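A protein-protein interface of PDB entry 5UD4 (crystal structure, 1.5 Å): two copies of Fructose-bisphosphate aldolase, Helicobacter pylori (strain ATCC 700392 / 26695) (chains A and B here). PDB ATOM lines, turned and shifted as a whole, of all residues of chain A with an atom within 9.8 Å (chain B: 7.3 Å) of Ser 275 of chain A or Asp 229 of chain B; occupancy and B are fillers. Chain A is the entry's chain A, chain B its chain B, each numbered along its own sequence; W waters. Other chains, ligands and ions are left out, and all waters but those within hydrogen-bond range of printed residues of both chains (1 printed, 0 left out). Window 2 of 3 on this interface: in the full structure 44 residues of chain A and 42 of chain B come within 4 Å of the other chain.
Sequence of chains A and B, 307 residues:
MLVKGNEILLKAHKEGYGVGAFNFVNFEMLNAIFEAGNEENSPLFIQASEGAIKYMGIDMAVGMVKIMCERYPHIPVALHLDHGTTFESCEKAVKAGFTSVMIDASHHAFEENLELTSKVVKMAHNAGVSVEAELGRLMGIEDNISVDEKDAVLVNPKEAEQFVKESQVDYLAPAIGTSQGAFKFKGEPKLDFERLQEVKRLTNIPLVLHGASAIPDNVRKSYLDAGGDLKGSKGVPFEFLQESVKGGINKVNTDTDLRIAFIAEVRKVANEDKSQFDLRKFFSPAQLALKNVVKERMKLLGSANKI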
ATOM      1  N   VAL A 269     -18.296  -9.124 -14.321  1.00  0.00           N
ATOM      2  CA  VAL A 269     -17.228  -8.124 -14.350  1.00  0.00           C
ATOM      3  C   VAL A 269     -17.117  -7.443 -12.996  1.00  0.00           C
ATOM      4  O   VAL A 269     -16.016  -7.260 -12.459  1.00  0.00           O
ATOM      5  CB  VAL A 269     -17.469  -7.103 -15.478  1.00  0.00           C
ATOM      6  CG1 VAL A 269     -16.518  -5.925 -15.348  1.00  0.00           C
ATOM      7  CG2 VAL A 269     -17.307  -7.771 -16.838  1.00  0.00           C
ATOM      8  N   ALA A 270     -18.253  -7.062 -12.417  1.00  0.00           N
ATOM      9  CA  ALA A 270     -18.227  -6.381 -11.127  1.00  0.00           C
ATOM     10  C   ALA A 270     -17.582  -7.259 -10.064  1.00  0.00           C
ATOM     11  O   ALA A 270     -16.838  -6.764  -9.206  1.00  0.00           O
ATOM     12  CB  ALA A 270     -19.646  -6.002 -10.710  1.00  0.00           C
ATOM     13  N   ASN A 271     -17.846  -8.570 -10.125  1.00  0.00           N
ATOM     14  CA  ASN A 271     -17.320  -9.514  -9.141  1.00  0.00           C
ATOM     15  C   ASN A 271     -15.817  -9.696  -9.272  1.00  0.00           C
ATOM     16  O   ASN A 271     -15.106  -9.806  -8.263  1.00  0.00           O
ATOM     17  CB  ASN A 271     -17.988 -10.879  -9.311  1.00  0.00           C
ATOM     18  CG  ASN A 271     -19.440 -10.881  -8.942  1.00  0.00           C
ATOM     19  OD1 ASN A 271     -19.920 -10.004  -8.236  1.00  0.00           O
ATOM     20  ND2 ASN A 271     -20.151 -11.904  -9.394  1.00  0.00           N
ATOM     21  N   GLU A 272     -15.323  -9.799 -10.497  1.00  0.00           N
ATOM     22  CA  GLU A 272     -13.964 -10.259 -10.716  1.00  0.00           C
ATOM     23  C   GLU A 272     -12.946  -9.134 -10.717  1.00  0.00           C
ATOM     24  O   GLU A 272     -11.751  -9.409 -10.582  1.00  0.00           O
ATOM     25  CB  GLU A 272     -13.873 -11.028 -12.028  1.00  0.00           C
ATOM     26  CG  GLU A 272     -14.797 -12.251 -12.037  1.00  0.00           C
ATOM     27  CD  GLU A 272     -14.630 -13.120 -13.252  1.00  0.00           C
ATOM     28  OE1 GLU A 272     -14.893 -14.338 -13.134  1.00  0.00           O
ATOM     29  OE2 GLU A 272     -14.237 -12.602 -14.316  1.00  0.00           O
ATOM     30  N   ASP A 273     -13.379  -7.878 -10.861  1.00  0.00           N
ATOM     31  CA  ASP A 273     -12.448  -6.745 -10.765  1.00  0.00           C
ATOM     32  C   ASP A 273     -13.148  -5.580 -10.066  1.00  0.00           C
ATOM     33  O   ASP A 273     -13.899  -4.828 -10.693  1.00  0.00           O
ATOM     34  CB  ASP A 273     -11.934  -6.335 -12.136  1.00  0.00           C
ATOM     35  CG  ASP A 273     -10.853  -5.285 -12.054  1.00  0.00           C
ATOM     36  OD1 ASP A 273     -10.597  -4.799 -10.935  1.00  0.00           O
ATOM     37  OD2 ASP A 273     -10.250  -4.958 -13.102  1.00  0.00           O
ATOM     38  N   LYS A 274     -12.866  -5.414  -8.773  1.00  0.00           N
ATOM     39  CA  LYS A 274     -13.463  -4.329  -8.000  1.00  0.00           C
ATOM     40  C   LYS A 274     -12.967  -2.955  -8.440  1.00  0.00           C
ATOM     41  O   LYS A 274     -13.598  -1.950  -8.109  1.00  0.00           O
ATOM     42  CB  LYS A 274     -13.184  -4.534  -6.507  1.00  0.00           C
ATOM     43  CG  LYS A 274     -13.821  -5.798  -5.917  1.00  0.00           C
ATOM     44  CD  LYS A 274     -15.299  -5.919  -6.299  1.00  0.00           C
ATOM     45  CE  LYS A 274     -15.995  -7.051  -5.574  1.00  0.00           C
ATOM     46  NZ  LYS A 274     -17.442  -7.038  -5.918  1.00  0.00           N
ATOM     47  N   SER A 275     -11.855  -2.889  -9.163  1.00  0.00           N
ATOM     48  CA  SER A 275     -11.326  -1.618  -9.619  1.00  0.00           C
ATOM     49  C   SER A 275     -11.879  -1.206 -10.978  1.00  0.00           C
ATOM     50  O   SER A 275     -11.572  -0.113 -11.440  1.00  0.00           O
ATOM     51  CB  SER A 275      -9.792  -1.671  -9.681  1.00  0.00           C
ATOM     52  OG  SER A 275      -9.358  -2.401 -10.813  1.00  0.00           O
ATOM     53  N   GLN A 276     -12.699  -2.034 -11.618  1.00  0.00           N
ATOM     54  CA  GLN A 276     -13.146  -1.764 -12.983  1.00  0.00           C
ATOM     55  C   GLN A 276     -14.332  -0.798 -13.003  1.00  0.00           C
ATOM     56  O   GLN A 276     -15.397  -1.089 -12.442  1.00  0.00           O
ATOM     57  CB  GLN A 276     -13.536  -3.070 -13.668  1.00  0.00           C
ATOM     58  CG  GLN A 276     -13.936  -2.885 -15.115  1.00  0.00           C
ATOM     59  CD  GLN A 276     -12.804  -2.335 -15.961  1.00  0.00           C
ATOM     60  OE1 GLN A 276     -12.780  -1.147 -16.300  1.00  0.00           O
ATOM     61  NE2 GLN A 276     -11.886  -3.204 -16.338  1.00  0.00           N
ATOM     62  N   PHE A 277     -14.179   0.318 -13.717  1.00  0.00           N
ATOM     63  CA  PHE A 277     -15.315   1.213 -13.908  1.00  0.00           C
ATOM     64  C   PHE A 277     -15.419   1.761 -15.331  1.00  0.00           C
ATOM     65  O   PHE A 277     -16.159   2.731 -15.563  1.00  0.00           O
ATOM     66  CB  PHE A 277     -15.291   2.348 -12.898  1.00  0.00           C
ATOM     67  CG  PHE A 277     -13.969   3.072 -12.802  1.00  0.00           C
ATOM     68  CD1 PHE A 277     -13.593   3.993 -13.763  1.00  0.00           C
ATOM     69  CD2 PHE A 277     -13.116   2.827 -11.749  1.00  0.00           C
ATOM     70  CE1 PHE A 277     -12.379   4.669 -13.664  1.00  0.00           C
ATOM     71  CE2 PHE A 277     -11.911   3.498 -11.640  1.00  0.00           C
ATOM     72  CZ  PHE A 277     -11.542   4.409 -12.606  1.00  0.00           C
ATOM     73  N   ASP A 278     -14.737   1.153 -16.296  1.00  0.00           N
ATOM     74  CA  ASP A 278     -14.972   1.462 -17.699  1.00  0.00           C
ATOM     75  C   ASP A 278     -16.254   0.772 -18.143  1.00  0.00           C
ATOM     76  O   ASP A 278     -16.317  -0.460 -18.164  1.00  0.00           O
ATOM     77  CB  ASP A 278     -13.784   1.000 -18.529  1.00  0.00           C
ATOM     78  CG  ASP A 278     -13.892   1.364 -19.990  1.00  0.00           C
ATOM     79  OD1 ASP A 278     -14.983   1.678 -20.502  1.00  0.00           O
ATOM     80  OD2 ASP A 278     -12.841   1.318 -20.653  1.00  0.00           O
ATOM     81  N   LEU A 279     -17.267   1.570 -18.506  1.00  0.00           N
ATOM     82  CA  LEU A 279     -18.568   1.007 -18.868  1.00  0.00           C
ATOM     83  C   LEU A 279     -18.428  -0.027 -19.977  1.00  0.00           C
ATOM     84  O   LEU A 279     -19.130  -1.045 -19.976  1.00  0.00           O
ATOM     85  CB  LEU A 279     -19.535   2.121 -19.296  1.00  0.00           C
ATOM     86  CG  LEU A 279     -20.326   2.859 -18.198  1.00  0.00           C
ATOM     87  CD1 LEU A 279     -19.417   3.704 -17.310  1.00  0.00           C
ATOM     88  CD2 LEU A 279     -21.372   3.734 -18.817  1.00  0.00           C
ATOM     89  N   LYS A 281     -16.127  -2.134 -20.532  1.00  0.00           N
ATOM     90  CA  LYS A 281     -15.618  -3.411 -20.056  1.00  0.00           C
ATOM     91  C   LYS A 281     -16.724  -4.256 -19.433  1.00  0.00           C
ATOM     92  O   LYS A 281     -16.620  -5.487 -19.409  1.00  0.00           O
ATOM     93  CB  LYS A 281     -14.492  -3.160 -19.060  1.00  0.00           C
ATOM     94  CG  LYS A 281     -13.249  -2.554 -19.695  1.00  0.00           C
ATOM     95  CD  LYS A 281     -12.366  -3.627 -20.248  1.00  0.00           C
ATOM     96  CE  LYS A 281     -11.088  -3.056 -20.831  1.00  0.00           C
ATOM     97  NZ  LYS A 281     -10.212  -4.155 -21.336  1.00  0.00           N
ATOM     98  N   PHE A 282     -17.777  -3.613 -18.927  1.00  0.00           N
ATOM     99  CA  PHE A 282     -18.964  -4.320 -18.458  1.00  0.00           C
ATOM    100  C   PHE A 282     -19.858  -4.729 -19.616  1.00  0.00           C
ATOM    101  O   PHE A 282     -20.359  -5.860 -19.653  1.00  0.00           O
ATOM    102  CB  PHE A 282     -19.785  -3.446 -17.508  1.00  0.00           C
ATOM    103  CG  PHE A 282     -19.164  -3.233 -16.169  1.00  0.00           C
ATOM    104  CD1 PHE A 282     -18.225  -2.224 -15.989  1.00  0.00           C
ATOM    105  CD2 PHE A 282     -19.515  -4.019 -15.080  1.00  0.00           C
ATOM    106  CE1 PHE A 282     -17.653  -2.010 -14.764  1.00  0.00           C
ATOM    107  CE2 PHE A 282     -18.947  -3.801 -13.858  1.00  0.00           C
ATOM    108  CZ  PHE A 282     -18.010  -2.798 -13.698  1.00  0.00           C
ATOM    109  N   PHE B 183      -5.552   7.994 -10.998  1.00  0.00           N
ATOM    110  CA  PHE B 183      -4.304   7.924 -10.235  1.00  0.00           C
ATOM    111  C   PHE B 183      -3.362   9.017 -10.730  1.00  0.00           C
ATOM    112  O   PHE B 183      -2.308   8.747 -11.324  1.00  0.00           O
ATOM    113  CB  PHE B 183      -3.689   6.516 -10.358  1.00  0.00           C
ATOM    114  CG  PHE B 183      -4.684   5.418 -10.152  1.00  0.00           C
ATOM    115  CD1 PHE B 183      -5.102   5.074  -8.876  1.00  0.00           C
ATOM    116  CD2 PHE B 183      -5.224   4.750 -11.230  1.00  0.00           C
ATOM    117  CE1 PHE B 183      -6.033   4.074  -8.687  1.00  0.00           C
ATOM    118  CE2 PHE B 183      -6.160   3.750 -11.045  1.00  0.00           C
ATOM    119  CZ  PHE B 183      -6.559   3.409  -9.776  1.00  0.00           C
ATOM    120  N   TYR B 223     -18.665   4.558  -4.406  1.00  0.00           N
ATOM    121  CA  TYR B 223     -17.989   3.457  -5.078  1.00  0.00           C
ATOM    122  C   TYR B 223     -17.475   2.437  -4.064  1.00  0.00           C
ATOM    123  O   TYR B 223     -17.659   1.224  -4.237  1.00  0.00           O
ATOM    124  CB  TYR B 223     -16.856   4.009  -5.948  1.00  0.00           C
ATOM    125  CG  TYR B 223     -16.331   3.005  -6.905  1.00  0.00           C
ATOM    126  CD1 TYR B 223     -17.025   2.703  -8.065  1.00  0.00           C
ATOM    127  CD2 TYR B 223     -15.152   2.333  -6.650  1.00  0.00           C
ATOM    128  CE1 TYR B 223     -16.553   1.752  -8.952  1.00  0.00           C
ATOM    129  CE2 TYR B 223     -14.668   1.387  -7.524  1.00  0.00           C
ATOM    130  CZ  TYR B 223     -15.374   1.095  -8.673  1.00  0.00           C
ATOM    131  OH  TYR B 223     -14.913   0.148  -9.545  1.00  0.00           O
ATOM    132  N   LEU B 224     -16.872   2.912  -2.972  1.00  0.00           N
ATOM    133  CA  LEU B 224     -16.341   2.007  -1.960  1.00  0.00           C
ATOM    134  C   LEU B 224     -17.460   1.295  -1.203  1.00  0.00           C
ATOM    135  O   LEU B 224     -17.332   0.108  -0.875  1.00  0.00           O
ATOM    136  CB  LEU B 224     -15.445   2.775  -0.986  1.00  0.00           C
ATOM    137  CG  LEU B 224     -14.205   3.524  -1.489  1.00  0.00           C
ATOM    138  CD1 LEU B 224     -13.173   3.642  -0.363  1.00  0.00           C
ATOM    139  CD2 LEU B 224     -13.574   2.941  -2.739  1.00  0.00           C
ATOM    140  N   ALA B 226     -20.143   0.280  -2.280  1.00  0.00           N
ATOM    141  CA  ALA B 226     -20.663  -0.764  -3.147  1.00  0.00           C
ATOM    142  C   ALA B 226     -19.636  -1.861  -3.429  1.00  0.00           C
ATOM    143  O   ALA B 226     -19.845  -2.673  -4.337  1.00  0.00           O
ATOM    144  CB  ALA B 226     -21.149  -0.149  -4.454  1.00  0.00           C
ATOM    145  N   GLY B 227     -18.532  -1.888  -2.689  1.00  0.00           N
ATOM    146  CA  GLY B 227     -17.538  -2.925  -2.842  1.00  0.00           C
ATOM    147  C   GLY B 227     -16.413  -2.591  -3.787  1.00  0.00           C
ATOM    148  O   GLY B 227     -15.511  -3.415  -3.962  1.00  0.00           O
ATOM    149  N   GLY B 228     -16.429  -1.413  -4.392  1.00  0.00           N
ATOM    150  CA  GLY B 228     -15.403  -1.069  -5.344  1.00  0.00           C
ATOM    151  C   GLY B 228     -14.096  -0.711  -4.676  1.00  0.00           C
ATOM    152  O   GLY B 228     -14.043  -0.396  -3.489  1.00  0.00           O
ATOM    153  N   ASP B 229     -13.025  -0.788  -5.461  1.00  0.00           N
ATOM    154  CA  ASP B 229     -11.668  -0.531  -4.993  1.00  0.00           C
ATOM    155  C   ASP B 229     -11.088   0.635  -5.776  1.00  0.00           C
ATOM    156  O   ASP B 229     -11.012   0.582  -7.008  1.00  0.00           O
ATOM    157  CB  ASP B 229     -10.794  -1.777  -5.163  1.00  0.00           C
ATOM    158  CG  ASP B 229      -9.406  -1.615  -4.563  1.00  0.00           C
ATOM    159  OD1 ASP B 229      -9.095  -0.534  -4.018  1.00  0.00           O
ATOM    160  OD2 ASP B 229      -8.626  -2.589  -4.630  1.00  0.00           O
ATOM    161  N   LEU B 230     -10.686   1.683  -5.067  1.00  0.00           N
ATOM    162  CA  LEU B 230     -10.009   2.835  -5.658  1.00  0.00           C
ATOM    163  C   LEU B 230      -8.690   3.095  -4.945  1.00  0.00           C
ATOM    164  O   LEU B 230      -8.303   4.246  -4.709  1.00  0.00           O
ATOM    165  CB  LEU B 230     -10.891   4.079  -5.612  1.00  0.00           C
ATOM    166  CG  LEU B 230     -12.130   4.070  -6.506  1.00  0.00           C
ATOM    167  CD1 LEU B 230     -13.108   5.108  -6.024  1.00  0.00           C
ATOM    168  CD2 LEU B 230     -11.754   4.331  -7.938  1.00  0.00           C
ATOM    169  N   LYS B 231      -7.975   2.028  -4.604  1.00  0.00           N
ATOM    170  CA  LYS B 231      -6.755   2.145  -3.813  1.00  0.00           C
ATOM    171  C   LYS B 231      -5.746   3.032  -4.526  1.00  0.00           C
ATOM    172  O   LYS B 231      -5.374   2.767  -5.674  1.00  0.00           O
ATOM    173  CB  LYS B 231      -6.157   0.762  -3.563  1.00  0.00           C
ATOM    174  CG  LYS B 231      -4.816   0.770  -2.844  1.00  0.00           C
ATOM    175  CD  LYS B 231      -4.290  -0.642  -2.670  1.00  0.00           C
ATOM    176  CE  LYS B 231      -2.988  -0.660  -1.883  1.00  0.00           C
ATOM    177  NZ  LYS B 231      -1.873  -0.031  -2.637  1.00  0.00           N
ATOM    178  N   GLY B 232      -5.293   4.077  -3.832  1.00  0.00           N
ATOM    179  CA  GLY B 232      -4.278   4.963  -4.350  1.00  0.00           C
ATOM    180  C   GLY B 232      -4.790   6.094  -5.216  1.00  0.00           C
ATOM    181  O   GLY B 232      -3.985   6.931  -5.658  1.00  0.00           O
ATOM    182  N   SER B 233      -6.095   6.158  -5.472  1.00  0.00           N
ATOM    183  CA  SER B 233      -6.599   7.148  -6.406  1.00  0.00           C
ATOM    184  C   SER B 233      -6.459   8.553  -5.831  1.00  0.00           C
ATOM    185  O   SER B 233      -6.492   8.766  -4.612  1.00  0.00           O
ATOM    186  CB  SER B 233      -8.057   6.864  -6.745  1.00  0.00           C
ATOM    187  OG  SER B 233      -8.833   6.971  -5.573  1.00  0.00           O
ATOM    188  N   ILE B 260     -17.003   6.511 -12.438  1.00  0.00           N
ATOM    189  CA  ILE B 260     -17.040   5.998 -11.071  1.00  0.00           C
ATOM    190  C   ILE B 260     -18.440   6.171 -10.490  1.00  0.00           C
ATOM    191  O   ILE B 260     -18.993   5.258  -9.871  1.00  0.00           O
ATOM    192  CB  ILE B 260     -15.976   6.687 -10.201  1.00  0.00           C
ATOM    193  CG1 ILE B 260     -14.561   6.401 -10.743  1.00  0.00           C
ATOM    194  CG2 ILE B 260     -16.099   6.234  -8.738  1.00  0.00           C
ATOM    195  CD1 ILE B 260     -13.476   7.199 -10.049  1.00  0.00           C
ATOM    196  N   ILE B 263     -20.841   3.595 -12.234  1.00  0.00           N
ATOM    197  CA  ILE B 263     -20.632   2.185 -11.928  1.00  0.00           C
ATOM    198  C   ILE B 263     -20.838   1.905 -10.438  1.00  0.00           C
ATOM    199  O   ILE B 263     -21.219   0.791 -10.066  1.00  0.00           O
ATOM    200  CB  ILE B 263     -19.242   1.734 -12.427  1.00  0.00           C
ATOM    201  CG1 ILE B 263     -19.206   1.733 -13.963  1.00  0.00           C
ATOM    202  CG2 ILE B 263     -18.839   0.375 -11.863  1.00  0.00           C
ATOM    203  CD1 ILE B 263     -20.159   0.722 -14.648  1.00  0.00           C
ATOM    204  N   ARG B 267     -22.962  -1.342  -9.302  1.00  0.00           N
ATOM    205  CA  ARG B 267     -22.475  -2.306  -8.318  1.00  0.00           C
ATOM    206  C   ARG B 267     -23.451  -2.440  -7.160  1.00  0.00           C
ATOM    207  O   ARG B 267     -23.715  -3.551  -6.668  1.00  0.00           O
ATOM    208  CB  ARG B 267     -21.095  -1.872  -7.810  1.00  0.00           C
ATOM    209  CG  ARG B 267     -19.995  -2.000  -8.839  1.00  0.00           C
ATOM    210  CD  ARG B 267     -18.627  -1.543  -8.283  1.00  0.00           C
ATOM    211  NE  ARG B 267     -17.564  -1.784  -9.251  1.00  0.00           N
ATOM    212  CZ  ARG B 267     -16.930  -2.942  -9.417  1.00  0.00           C
ATOM    213  NH1 ARG B 267     -17.226  -4.000  -8.672  1.00  0.00           N
ATOM    214  NH2 ARG B 267     -16.000  -3.044 -10.351  1.00  0.00           N
HETATM  215  O   HOH W   1     -18.809  -4.395  -6.314  1.00  0.00           O
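No position is printed for both chains. Of the 19 pairs that touch across the chains among the printed residues, none has its exchanged pair printed and touching as well.
Gly 227 of chain B touches Lys 274 of chain A. O of Lys 274 of chain A touches CA of Gly 228 of chain B, at 3.4 Å. Ser 275 of chain A touches Asp 229 of chain B (CA to O, 3.4 Å). O of Gln 276 of chain A touches CG2 of Ile 263 of chain B (3.8 Å). OH of Tyr 223 of chain B touches CD2 of Phe 277 of chain A, at 3.9 Å. Phe 277 of chain A touches Leu 230 of chain B. CG of Phe 277 of chain A touches CG1 of Ile 260 of chain B (3.96 Å). CG1 of Ile 263 of chain B touches O of Phe 277 of chain A (3.6 Å). Leu 279 of chain A touches Ile 263 of chain B. Ile 263 of chain B touches Phe 282 of chain A.
Hydrophobic or aromatic side chains of chain B that line the printed part of chain A: Tyr 223, Leu 230, Ile 260 and Ile 263. Among the printed residues, 19 pairs touch across the chains. Among the printed residues, no Asp or Glu carboxylate lies within 4 Å of a Lys or Arg side-chain nitrogen of the other chain.
Of chain B, only Tyr 223 (3.6 Å) and Asp 229 (3.4 Å) come within 4 Å of Ser 275 of chain A. Of the printed residues of chain B, Gln 276 of chain A touches Tyr 223, Ile 263 and Arg 267. Printed residues of chain B within 4 Å of Phe 277 of chain A: Tyr 223, Leu 230, Ile 260 and Ile 263. Printed residues of chain B within 4 Å of Leu 279 of chain A: Ile 263. Lys 281 of chain A touches none of the printed residues of chain B. Of chain A, only Lys 274 comes within 4 Å of Gly 228 of chain B. Of the printed residues of chain A, Asp 229 of chain B touches Lys 274 (2.9 Å) and Ser 275 (3.4 Å). Of chain A, only Phe 277 comes within 4 Å of Leu 230 of chain B. Printed residues of chain A within 4 Å of Ile 260 of chain B: Phe 277. Printed residues of chain A within 4 Å of Ile 263 of chain B: Gln 276, Phe 277, Leu 279 and Phe 282. The nearest printed residue of chain A that does not touch Asp 229 of chain B is Phe 277 of chain A (5.5 Å).
Water W1 lies within hydrogen-bond range of the backbone carbonyl oxygen of Ala 226 of chain B, the guanidinium group of Arg 267 of chain B and the side-chain amino group of Lys 274 of chain A.
The backbone carbonyl oxygen (O) of Ala 270 of chain A sits at hydrogen-bond distance from the guanidinium group (NH1) of Arg 267 of chain B (2.8 Å). O of Asp 273 of chain A lies within hydrogen-bond range of NH2 of Arg 267 of chain B, 2.8 Å away. The backbone carbonyl oxygen (O) of Lys 274 of chain A lies within hydrogen-bond range of the side-chain hydroxyl (OH) of Tyr 223 of chain B. The backbone carbonyl oxygen (O) of Lys 274 of chain A is in hydrogen-bond range of the backbone NH (N) of Asp 229 of chain B (2.9 Å). O of Lys 274 of chain A is in hydrogen-bond range of NH2 of Arg 267 of chain B, at 3.5 Å. OH of Tyr 223 of chain B is in hydrogen-bond range of O of Gln 276 of chain A, at 3.2 Å. O of Gln 276 of chain A is in hydrogen-bond range of NH2 of Arg 267 of chain B.
The side-chain carboxylate of Asp 273 of chain A is in hydrogen-bond range of the side-chain hydroxyl of Ser 275 of chain A (2.7 Å). The side-chain amide oxygen of Gln 276 of chain A is in hydrogen-bond range of the backbone NH of Asp 278 of chain A (3.0 Å). The backbone carbonyl oxygen (O) of Tyr 223 of chain B is in hydrogen-bond range of the backbone NH (N) of Gly 228 of chain B, 2.9 Å away. NE of Arg 267 of chain B is in hydrogen-bond range of OH of Tyr 223 of chain B (3.3 Å). The backbone NH of Lys 231 of chain B lies within hydrogen-bond range of the side-chain carboxylate of Asp 229 of chain B, 2.9 Å away. The side-chain hydroxyl of Ser 233 of chain B lies within hydrogen-bond range of the backbone carbonyl oxygen of Leu 230 of chain B.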
